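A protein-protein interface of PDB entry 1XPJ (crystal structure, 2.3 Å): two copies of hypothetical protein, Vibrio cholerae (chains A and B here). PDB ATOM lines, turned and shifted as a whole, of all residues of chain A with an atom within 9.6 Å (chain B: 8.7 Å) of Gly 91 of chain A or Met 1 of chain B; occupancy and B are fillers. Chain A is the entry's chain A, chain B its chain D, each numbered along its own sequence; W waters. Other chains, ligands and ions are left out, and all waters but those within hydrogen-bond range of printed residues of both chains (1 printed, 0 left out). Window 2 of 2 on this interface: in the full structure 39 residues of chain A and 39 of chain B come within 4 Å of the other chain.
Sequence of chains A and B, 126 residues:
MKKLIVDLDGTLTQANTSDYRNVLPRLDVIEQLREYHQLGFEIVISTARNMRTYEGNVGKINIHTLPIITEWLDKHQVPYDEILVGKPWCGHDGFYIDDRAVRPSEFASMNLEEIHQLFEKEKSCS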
ATOM      1  N   ALA A  48      -1.230  27.156  -5.922  1.00  0.00           N
ATOM      2  CA  ALA A  48      -0.913  27.341  -4.501  1.00  0.00           C
ATOM      3  C   ALA A  48      -0.706  28.817  -4.099  1.00  0.00           C
ATOM      4  O   ALA A  48      -0.308  29.102  -2.956  1.00  0.00           O
ATOM      5  CB  ALA A  48       0.307  26.519  -4.127  1.00  0.00           C
ATOM      6  N   MET A  51      -0.915  30.632  -0.503  1.00  0.00           N
ATOM      7  CA  MET A  51      -0.967  29.623   0.541  1.00  0.00           C
ATOM      8  C   MET A  51       0.089  29.907   1.614  1.00  0.00           C
ATOM      9  O   MET A  51      -0.145  29.728   2.794  1.00  0.00           O
ATOM     10  CB  MET A  51      -0.802  28.190   0.046  1.00  0.00           C
ATOM     11  CG  MET A  51      -2.012  27.688  -0.739  1.00  0.00           C
ATOM     12  SD  MET A  51      -2.904  26.476   0.240  1.00  0.00           S
ATOM     13  CE  MET A  51      -4.244  27.531   0.813  1.00  0.00           C
ATOM     14  N   ARG A  52       1.259  30.385   1.192  1.00  0.00           N
ATOM     15  CA  ARG A  52       2.305  30.757   2.146  1.00  0.00           C
ATOM     16  C   ARG A  52       1.835  31.965   2.965  1.00  0.00           C
ATOM     17  O   ARG A  52       1.690  31.865   4.185  1.00  0.00           O
ATOM     18  CB  ARG A  52       3.636  31.043   1.444  1.00  0.00           C
ATOM     19  CG  ARG A  52       4.825  30.951   2.366  1.00  0.00           C
ATOM     20  CD  ARG A  52       5.609  32.237   2.532  1.00  0.00           C
ATOM     21  NE  ARG A  52       6.705  32.338   1.572  1.00  0.00           N
ATOM     22  CZ  ARG A  52       7.891  32.887   1.844  1.00  0.00           C
ATOM     23  NH1 ARG A  52       8.146  33.385   3.057  1.00  0.00           N
ATOM     24  NH2 ARG A  52       8.828  32.934   0.899  1.00  0.00           N
ATOM     25  N   LYS A  87      -4.113  24.636  -3.659  1.00  0.00           N
ATOM     26  CA  LYS A  87      -3.138  23.597  -3.987  1.00  0.00           C
ATOM     27  C   LYS A  87      -2.101  23.572  -2.861  1.00  0.00           C
ATOM     28  O   LYS A  87      -1.706  24.637  -2.364  1.00  0.00           O
ATOM     29  CB  LYS A  87      -2.444  23.959  -5.302  1.00  0.00           C
ATOM     30  CG  LYS A  87      -1.730  22.812  -5.988  1.00  0.00           C
ATOM     31  CD  LYS A  87      -0.653  23.340  -6.931  1.00  0.00           C
ATOM     32  CE  LYS A  87      -0.002  22.221  -7.716  1.00  0.00           C
ATOM     33  NZ  LYS A  87       0.739  22.766  -8.885  1.00  0.00           N
ATOM     34  N   PRO A  88      -1.662  22.375  -2.462  1.00  0.00           N
ATOM     35  CA  PRO A  88      -0.581  22.228  -1.477  1.00  0.00           C
ATOM     36  C   PRO A  88       0.678  22.979  -1.918  1.00  0.00           C
ATOM     37  O   PRO A  88       1.101  22.817  -3.065  1.00  0.00           O
ATOM     38  CB  PRO A  88      -0.313  20.713  -1.477  1.00  0.00           C
ATOM     39  CG  PRO A  88      -1.558  20.102  -1.985  1.00  0.00           C
ATOM     40  CD  PRO A  88      -2.158  21.070  -2.939  1.00  0.00           C
ATOM     41  N   TRP A  89       1.234  23.792  -1.027  1.00  0.00           N
ATOM     42  CA  TRP A  89       2.487  24.514  -1.276  1.00  0.00           C
ATOM     43  C   TRP A  89       3.676  23.634  -0.892  1.00  0.00           C
ATOM     44  O   TRP A  89       3.766  23.176   0.239  1.00  0.00           O
ATOM     45  CB  TRP A  89       2.500  25.837  -0.482  1.00  0.00           C
ATOM     46  CG  TRP A  89       3.817  26.596  -0.447  1.00  0.00           C
ATOM     47  CD1 TRP A  89       4.454  27.076   0.665  1.00  0.00           C
ATOM     48  CD2 TRP A  89       4.633  26.978  -1.566  1.00  0.00           C
ATOM     49  NE1 TRP A  89       5.613  27.725   0.310  1.00  0.00           N
ATOM     50  CE2 TRP A  89       5.749  27.680  -1.053  1.00  0.00           C
ATOM     51  CE3 TRP A  89       4.537  26.799  -2.953  1.00  0.00           C
ATOM     52  CZ2 TRP A  89       6.759  28.196  -1.876  1.00  0.00           C
ATOM     53  CZ3 TRP A  89       5.541  27.312  -3.769  1.00  0.00           C
ATOM     54  CH2 TRP A  89       6.637  27.998  -3.226  1.00  0.00           C
ATOM     55  N   CYS A  90       4.573  23.407  -1.850  1.00  0.00           N
ATOM     56  CA  CYS A  90       5.774  22.595  -1.631  1.00  0.00           C
ATOM     57  C   CYS A  90       6.975  23.273  -0.958  1.00  0.00           C
ATOM     58  O   CYS A  90       7.952  22.595  -0.670  1.00  0.00           O
ATOM     59  CB  CYS A  90       6.253  21.939  -2.927  1.00  0.00           C
ATOM     60  SG  CYS A  90       6.604  23.081  -4.272  1.00  0.00           S
ATOM     61  N   GLY A  91       6.918  24.579  -0.701  1.00  0.00           N
ATOM     62  CA  GLY A  91       8.054  25.301  -0.118  1.00  0.00           C
ATOM     63  C   GLY A  91       9.066  25.672  -1.184  1.00  0.00           C
ATOM     64  O   GLY A  91       8.918  25.238  -2.330  1.00  0.00           O
ATOM     65  N   HIS A  92      10.087  26.456  -0.838  1.00  0.00           N
ATOM     66  CA  HIS A  92      11.105  26.857  -1.829  1.00  0.00           C
ATOM     67  C   HIS A  92      11.773  25.662  -2.523  1.00  0.00           C
ATOM     68  O   HIS A  92      11.937  25.662  -3.741  1.00  0.00           O
ATOM     69  CB  HIS A  92      12.201  27.753  -1.209  1.00  0.00           C
ATOM     70  CG  HIS A  92      13.174  28.318  -2.211  1.00  0.00           C
ATOM     71  ND1 HIS A  92      13.501  27.679  -3.389  1.00  0.00           N
ATOM     72  CD2 HIS A  92      13.894  29.466  -2.200  1.00  0.00           C
ATOM     73  CE1 HIS A  92      14.375  28.408  -4.060  1.00  0.00           C
ATOM     74  NE2 HIS A  92      14.629  29.499  -3.360  1.00  0.00           N
ATOM     75  N   ASP A  93      12.169  24.666  -1.739  1.00  0.00           N
ATOM     76  CA  ASP A  93      12.978  23.566  -2.248  1.00  0.00           C
ATOM     77  C   ASP A  93      12.173  22.327  -2.633  1.00  0.00           C
ATOM     78  O   ASP A  93      12.745  21.336  -3.095  1.00  0.00           O
ATOM     79  CB  ASP A  93      14.057  23.172  -1.224  1.00  0.00           C
ATOM     80  CG  ASP A  93      15.023  24.312  -0.895  1.00  0.00           C
ATOM     81  OD1 ASP A  93      15.327  25.147  -1.782  1.00  0.00           O
ATOM     82  OD2 ASP A  93      15.543  24.428   0.235  1.00  0.00           O
ATOM     83  N   GLY A  94      10.857  22.371  -2.452  1.00  0.00           N
ATOM     84  CA  GLY A  94      10.017  21.223  -2.754  1.00  0.00           C
ATOM     85  C   GLY A  94       9.679  21.045  -4.224  1.00  0.00           C
ATOM     86  O   GLY A  94      10.045  21.880  -5.065  1.00  0.00           O
ATOM     87  N   PHE A  95       8.968  19.958  -4.538  1.00  0.00           N
ATOM     88  CA  PHE A  95       8.477  19.725  -5.902  1.00  0.00           C
ATOM     89  C   PHE A  95       7.419  18.629  -5.967  1.00  0.00           C
ATOM     90  O   PHE A  95       7.171  17.904  -4.986  1.00  0.00           O
ATOM     91  CB  PHE A  95       9.624  19.456  -6.909  1.00  0.00           C
ATOM     92  CG  PHE A  95      10.569  18.307  -6.528  1.00  0.00           C
ATOM     93  CD1 PHE A  95      10.343  17.016  -6.992  1.00  0.00           C
ATOM     94  CD2 PHE A  95      11.690  18.537  -5.755  1.00  0.00           C
ATOM     95  CE1 PHE A  95      11.216  15.958  -6.654  1.00  0.00           C
ATOM     96  CE2 PHE A  95      12.568  17.508  -5.417  1.00  0.00           C
ATOM     97  CZ  PHE A  95      12.343  16.221  -5.871  1.00  0.00           C
ATOM     98  N   TYR A  96       6.791  18.522  -7.131  1.00  0.00           N
ATOM     99  CA  TYR A  96       5.738  17.558  -7.342  1.00  0.00           C
ATOM    100  C   TYR A  96       6.292  16.355  -8.088  1.00  0.00           C
ATOM    101  O   TYR A  96       7.170  16.520  -8.937  1.00  0.00           O
ATOM    102  CB  TYR A  96       4.585  18.216  -8.083  1.00  0.00           C
ATOM    103  CG  TYR A  96       4.042  19.409  -7.331  1.00  0.00           C
ATOM    104  CD1 TYR A  96       2.889  19.298  -6.545  1.00  0.00           C
ATOM    105  CD2 TYR A  96       4.691  20.661  -7.387  1.00  0.00           C
ATOM    106  CE1 TYR A  96       2.386  20.398  -5.830  1.00  0.00           C
ATOM    107  CE2 TYR A  96       4.200  21.768  -6.674  1.00  0.00           C
ATOM    108  CZ  TYR A  96       3.045  21.626  -5.898  1.00  0.00           C
ATOM    109  OH  TYR A  96       2.546  22.713  -5.193  1.00  0.00           O
ATOM    110  N   MET B   1      11.310  24.868   5.395  1.00  0.00           N
ATOM    111  CA  MET B   1      10.193  23.919   5.136  1.00  0.00           C
ATOM    112  C   MET B   1      10.178  23.494   3.671  1.00  0.00           C
ATOM    113  O   MET B   1      10.113  24.336   2.765  1.00  0.00           O
ATOM    114  CB  MET B   1       8.855  24.548   5.501  1.00  0.00           C
ATOM    115  CG  MET B   1       7.702  23.550   5.321  1.00  0.00           C
ATOM    116  SD  MET B   1       6.469  24.118   4.146  1.00  0.00           S
ATOM    117  CE  MET B   1       6.988  23.137   2.729  1.00  0.00           C
ATOM    118  N   LYS B   2      10.231  22.185   3.454  1.00  0.00           N
ATOM    119  CA  LYS B   2      10.301  21.619   2.113  1.00  0.00           C
ATOM    120  C   LYS B   2       9.530  20.313   2.055  1.00  0.00           C
ATOM    121  O   LYS B   2       9.721  19.432   2.889  1.00  0.00           O
ATOM    122  CB  LYS B   2      11.762  21.451   1.638  1.00  0.00           C
ATOM    123  CG  LYS B   2      12.663  20.632   2.557  1.00  0.00           C
ATOM    124  CD  LYS B   2      14.126  20.783   2.165  1.00  0.00           C
ATOM    125  CE  LYS B   2      15.039  20.509   3.343  1.00  0.00           C
ATOM    126  NZ  LYS B   2      15.981  19.397   3.050  1.00  0.00           N
ATOM    127  N   LYS B   3       8.640  20.221   1.076  1.00  0.00           N
ATOM    128  CA  LYS B   3       7.784  19.049   0.903  1.00  0.00           C
ATOM    129  C   LYS B   3       7.982  18.424  -0.481  1.00  0.00           C
ATOM    130  O   LYS B   3       8.290  19.113  -1.457  1.00  0.00           O
ATOM    131  CB  LYS B   3       6.289  19.403   1.088  1.00  0.00           C
ATOM    132  CG  LYS B   3       5.967  20.158   2.386  1.00  0.00           C
ATOM    133  CD  LYS B   3       4.548  19.881   2.871  1.00  0.00           C
ATOM    134  CE  LYS B   3       3.666  21.116   2.785  1.00  0.00           C
ATOM    135  NZ  LYS B   3       2.673  21.162   3.899  1.00  0.00           N
ATOM    136  N   LEU B   4       7.813  17.112  -0.537  1.00  0.00           N
ATOM    137  CA  LEU B   4       7.561  16.425  -1.775  1.00  0.00           C
ATOM    138  C   LEU B   4       6.053  16.158  -1.825  1.00  0.00           C
ATOM    139  O   LEU B   4       5.470  15.653  -0.851  1.00  0.00           O
ATOM    140  CB  LEU B   4       8.338  15.113  -1.825  1.00  0.00           C
ATOM    141  CG  LEU B   4       9.564  14.992  -2.735  1.00  0.00           C
ATOM    142  CD1 LEU B   4      10.347  16.304  -2.854  1.00  0.00           C
ATOM    143  CD2 LEU B   4      10.475  13.860  -2.231  1.00  0.00           C
ATOM    144  N   ILE B   5       5.433  16.544  -2.946  1.00  0.00           N
ATOM    145  CA  ILE B   5       4.030  16.239  -3.230  1.00  0.00           C
ATOM    146  C   ILE B   5       3.994  15.096  -4.246  1.00  0.00           C
ATOM    147  O   ILE B   5       4.343  15.284  -5.427  1.00  0.00           O
ATOM    148  CB  ILE B   5       3.273  17.495  -3.756  1.00  0.00           C
ATOM    149  CG1 ILE B   5       3.627  18.746  -2.950  1.00  0.00           C
ATOM    150  CG2 ILE B   5       1.741  17.260  -3.785  1.00  0.00           C
ATOM    151  CD1 ILE B   5       3.482  18.599  -1.444  1.00  0.00           C
ATOM    152  N   GLY B  40      15.373  15.644   5.279  1.00  0.00           N
ATOM    153  CA  GLY B  40      14.501  16.625   5.908  1.00  0.00           C
ATOM    154  C   GLY B  40      13.194  16.949   5.190  1.00  0.00           C
ATOM    155  O   GLY B  40      12.367  17.686   5.740  1.00  0.00           O
ATOM    156  N   PHE B  41      12.999  16.405   3.983  1.00  0.00           N
ATOM    157  CA  PHE B  41      11.765  16.614   3.211  1.00  0.00           C
ATOM    158  C   PHE B  41      10.578  15.927   3.860  1.00  0.00           C
ATOM    159  O   PHE B  41      10.670  14.766   4.244  1.00  0.00           O
ATOM    160  CB  PHE B  41      11.893  16.047   1.800  1.00  0.00           C
ATOM    161  CG  PHE B  41      12.755  16.859   0.880  1.00  0.00           C
ATOM    162  CD1 PHE B  41      12.180  17.679  -0.091  1.00  0.00           C
ATOM    163  CD2 PHE B  41      14.131  16.786   0.954  1.00  0.00           C
ATOM    164  CE1 PHE B  41      12.977  18.430  -0.966  1.00  0.00           C
ATOM    165  CE2 PHE B  41      14.923  17.533   0.097  1.00  0.00           C
ATOM    166  CZ  PHE B  41      14.346  18.351  -0.861  1.00  0.00           C
ATOM    167  N   GLU B  42       9.462  16.643   3.954  1.00  0.00           N
ATOM    168  CA  GLU B  42       8.187  16.070   4.351  1.00  0.00           C
ATOM    169  C   GLU B  42       7.548  15.436   3.133  1.00  0.00           C
ATOM    170  O   GLU B  42       7.670  15.965   2.025  1.00  0.00           O
ATOM    171  CB  GLU B  42       7.262  17.149   4.912  1.00  0.00           C
ATOM    172  CG  GLU B  42       7.819  17.879   6.141  1.00  0.00           C
ATOM    173  CD  GLU B  42       7.180  19.254   6.356  1.00  0.00           C
ATOM    174  OE1 GLU B  42       5.931  19.348   6.338  1.00  0.00           O
ATOM    175  OE2 GLU B  42       7.927  20.249   6.549  1.00  0.00           O
ATOM    176  N   VAL B  44       4.166  14.269   1.248  1.00  0.00           N
ATOM    177  CA  VAL B  44       2.724  14.422   1.146  1.00  0.00           C
ATOM    178  C   VAL B  44       2.240  13.561  -0.020  1.00  0.00           C
ATOM    179  O   VAL B  44       2.579  13.841  -1.169  1.00  0.00           O
ATOM    180  CB  VAL B  44       2.328  15.908   0.899  1.00  0.00           C
ATOM    181  CG1 VAL B  44       0.823  16.062   0.663  1.00  0.00           C
ATOM    182  CG2 VAL B  44       2.799  16.811   2.059  1.00  0.00           C
ATOM    183  N   GLU B  82       1.801  13.246   5.337  1.00  0.00           N
ATOM    184  CA  GLU B  82       0.427  13.681   5.076  1.00  0.00           C
ATOM    185  C   GLU B  82      -0.186  12.853   3.972  1.00  0.00           C
ATOM    186  O   GLU B  82       0.529  12.400   3.081  1.00  0.00           O
ATOM    187  CB  GLU B  82       0.389  15.145   4.624  1.00  0.00           C
ATOM    188  CG  GLU B  82       0.328  16.156   5.756  1.00  0.00           C
ATOM    189  CD  GLU B  82       0.732  17.549   5.309  1.00  0.00           C
ATOM    190  OE1 GLU B  82       1.696  18.095   5.873  1.00  0.00           O
ATOM    191  OE2 GLU B  82       0.077  18.109   4.397  1.00  0.00           O
ATOM    192  N   ARG B 100       7.604  22.888 -11.431  1.00  0.00           N
ATOM    193  CA  ARG B 100       8.293  22.085 -10.422  1.00  0.00           C
ATOM    194  C   ARG B 100       7.884  20.613 -10.459  1.00  0.00           C
ATOM    195  O   ARG B 100       7.966  19.932  -9.451  1.00  0.00           O
ATOM    196  CB  ARG B 100       8.087  22.643  -9.009  1.00  0.00           C
ATOM    197  CG  ARG B 100       8.383  24.119  -8.843  1.00  0.00           C
ATOM    198  CD  ARG B 100       9.842  24.453  -8.598  1.00  0.00           C
ATOM    199  NE  ARG B 100      10.359  23.841  -7.377  1.00  0.00           N
ATOM    200  CZ  ARG B 100      11.617  23.942  -6.963  1.00  0.00           C
ATOM    201  NH1 ARG B 100      12.494  24.644  -7.667  1.00  0.00           N
ATOM    202  NH2 ARG B 100      12.002  23.341  -5.842  1.00  0.00           N
HETATM  203  O   HOH W   1      12.021  24.831   0.959  1.00  0.00           O
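No position is printed for both chains.
Of the 16 pairs that touch across the chains among the printed residues, none has its exchanged pair printed and touching as well.
The backbone NH (N) of Val 44 of chain B is in hydrogen-bond range of the backbone carbonyl oxygen (O) of Leu 4 of chain B (2.8 Å).
The backbone NH (N) of Leu 4 of chain B lies within hydrogen-bond range of the backbone carbonyl oxygen (O) of Glu 42 of chain B (2.8 Å).
The backbone NH of Glu 42 of chain B sits at hydrogen-bond distance from the backbone carbonyl oxygen of Lys 2 of chain B (3.0 Å).
O of Gly 94 of chain A lies close to SG of Cys 90 of chain A, at 3.7 Å.
The side-chain hydroxyl of Tyr 96 of chain A is in hydrogen-bond range of the backbone carbonyl oxygen of Pro 88 of chain A.
OE1 of Glu 82 of chain B lies within salt-bridge range of NZ of Lys 3 of chain B (3.8 Å).
Hydrophobic or aromatic side chains of chain A that line the printed part of chain B: Phe 95 and Tyr 96.
Among the printed residues, no Asp or Glu carboxylate lies within 4 Å of a Lys or Arg side-chain nitrogen of the other chain.
Water W1 lies within hydrogen-bond range of the backbone carbonyl oxygen (O) of Met 1 of chain B (2.7 Å), the backbone NH (N) of Asp 93 of chain A (2.7 Å) and the backbone NH (N) of His 92 of chain A (3.1 Å).
Trp 89 of chain A touches Lys 3 of chain B (O to CE, 3.3 Å).
Cys 90 of chain A touches Met 1 of chain B.
Lys 2 of chain B touches Cys 90 of chain A (CA to O, 3.8 Å).
Gly 91 of chain A touches Met 1 of chain B.
Asp 93 of chain A touches Phe 41 of chain B.
Gly 94 of chain A touches Lys 3 of chain B.
CA of Leu 4 of chain B touches O of Phe 95 of chain A (3.6 Å).
Arg 100 of chain B touches Phe 95 of chain A.
Ile 5 of chain B touches Tyr 96 of chain A.
N of Lys 3 of chain B is in hydrogen-bond range of O of Cys 90 of chain A.
The guanidinium group (NH2) of Arg 100 of chain B sits at hydrogen-bond distance from the backbone carbonyl oxygen (O) of His 92 of chain A (3.1 Å).
The backbone NH of Tyr 96 of chain A lies within hydrogen-bond range of the backbone carbonyl oxygen of Arg 100 of chain B, at 3.0 Å.
The backbone carbonyl oxygen of Phe 95 of chain A lies within hydrogen-bond range of the backbone NH of Ile 5 of chain B (3.0 Å).
O of Gly 94 of chain A sits at hydrogen-bond distance from NH2 of Arg 100 of chain B (2.6 Å).
The backbone carbonyl oxygen (O) of Asp 93 of chain A sits close to the guanidinium group (NH2) of Arg 100 of chain B (3.5 Å).
N of Phe 95 of chain A is in hydrogen-bond range of O of Lys 3 of chain B (3.3 Å).
Of chain B, only Met 1 (3.7 Å) comes within 4 Å of Gly 91 of chain A.
Of the printed residues of chain A, Met 1 of chain B touches Cys 90 and Gly 91.
Of the printed residues of chain B, Trp 89 of chain A touches Lys 3.
Of the printed residues of chain B, Phe 95 of chain A touches Lys 3, Leu 4, Ile 5 and Arg 100.
Arg 52 of chain A touches none of the printed residues of chain B.
Ala 48 of chain A touches none of the printed residues of chain B.
The nearest printed residue of chain B that does not touch Cys 90 of chain A is Ile 5 of chain B (4.1 Å).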
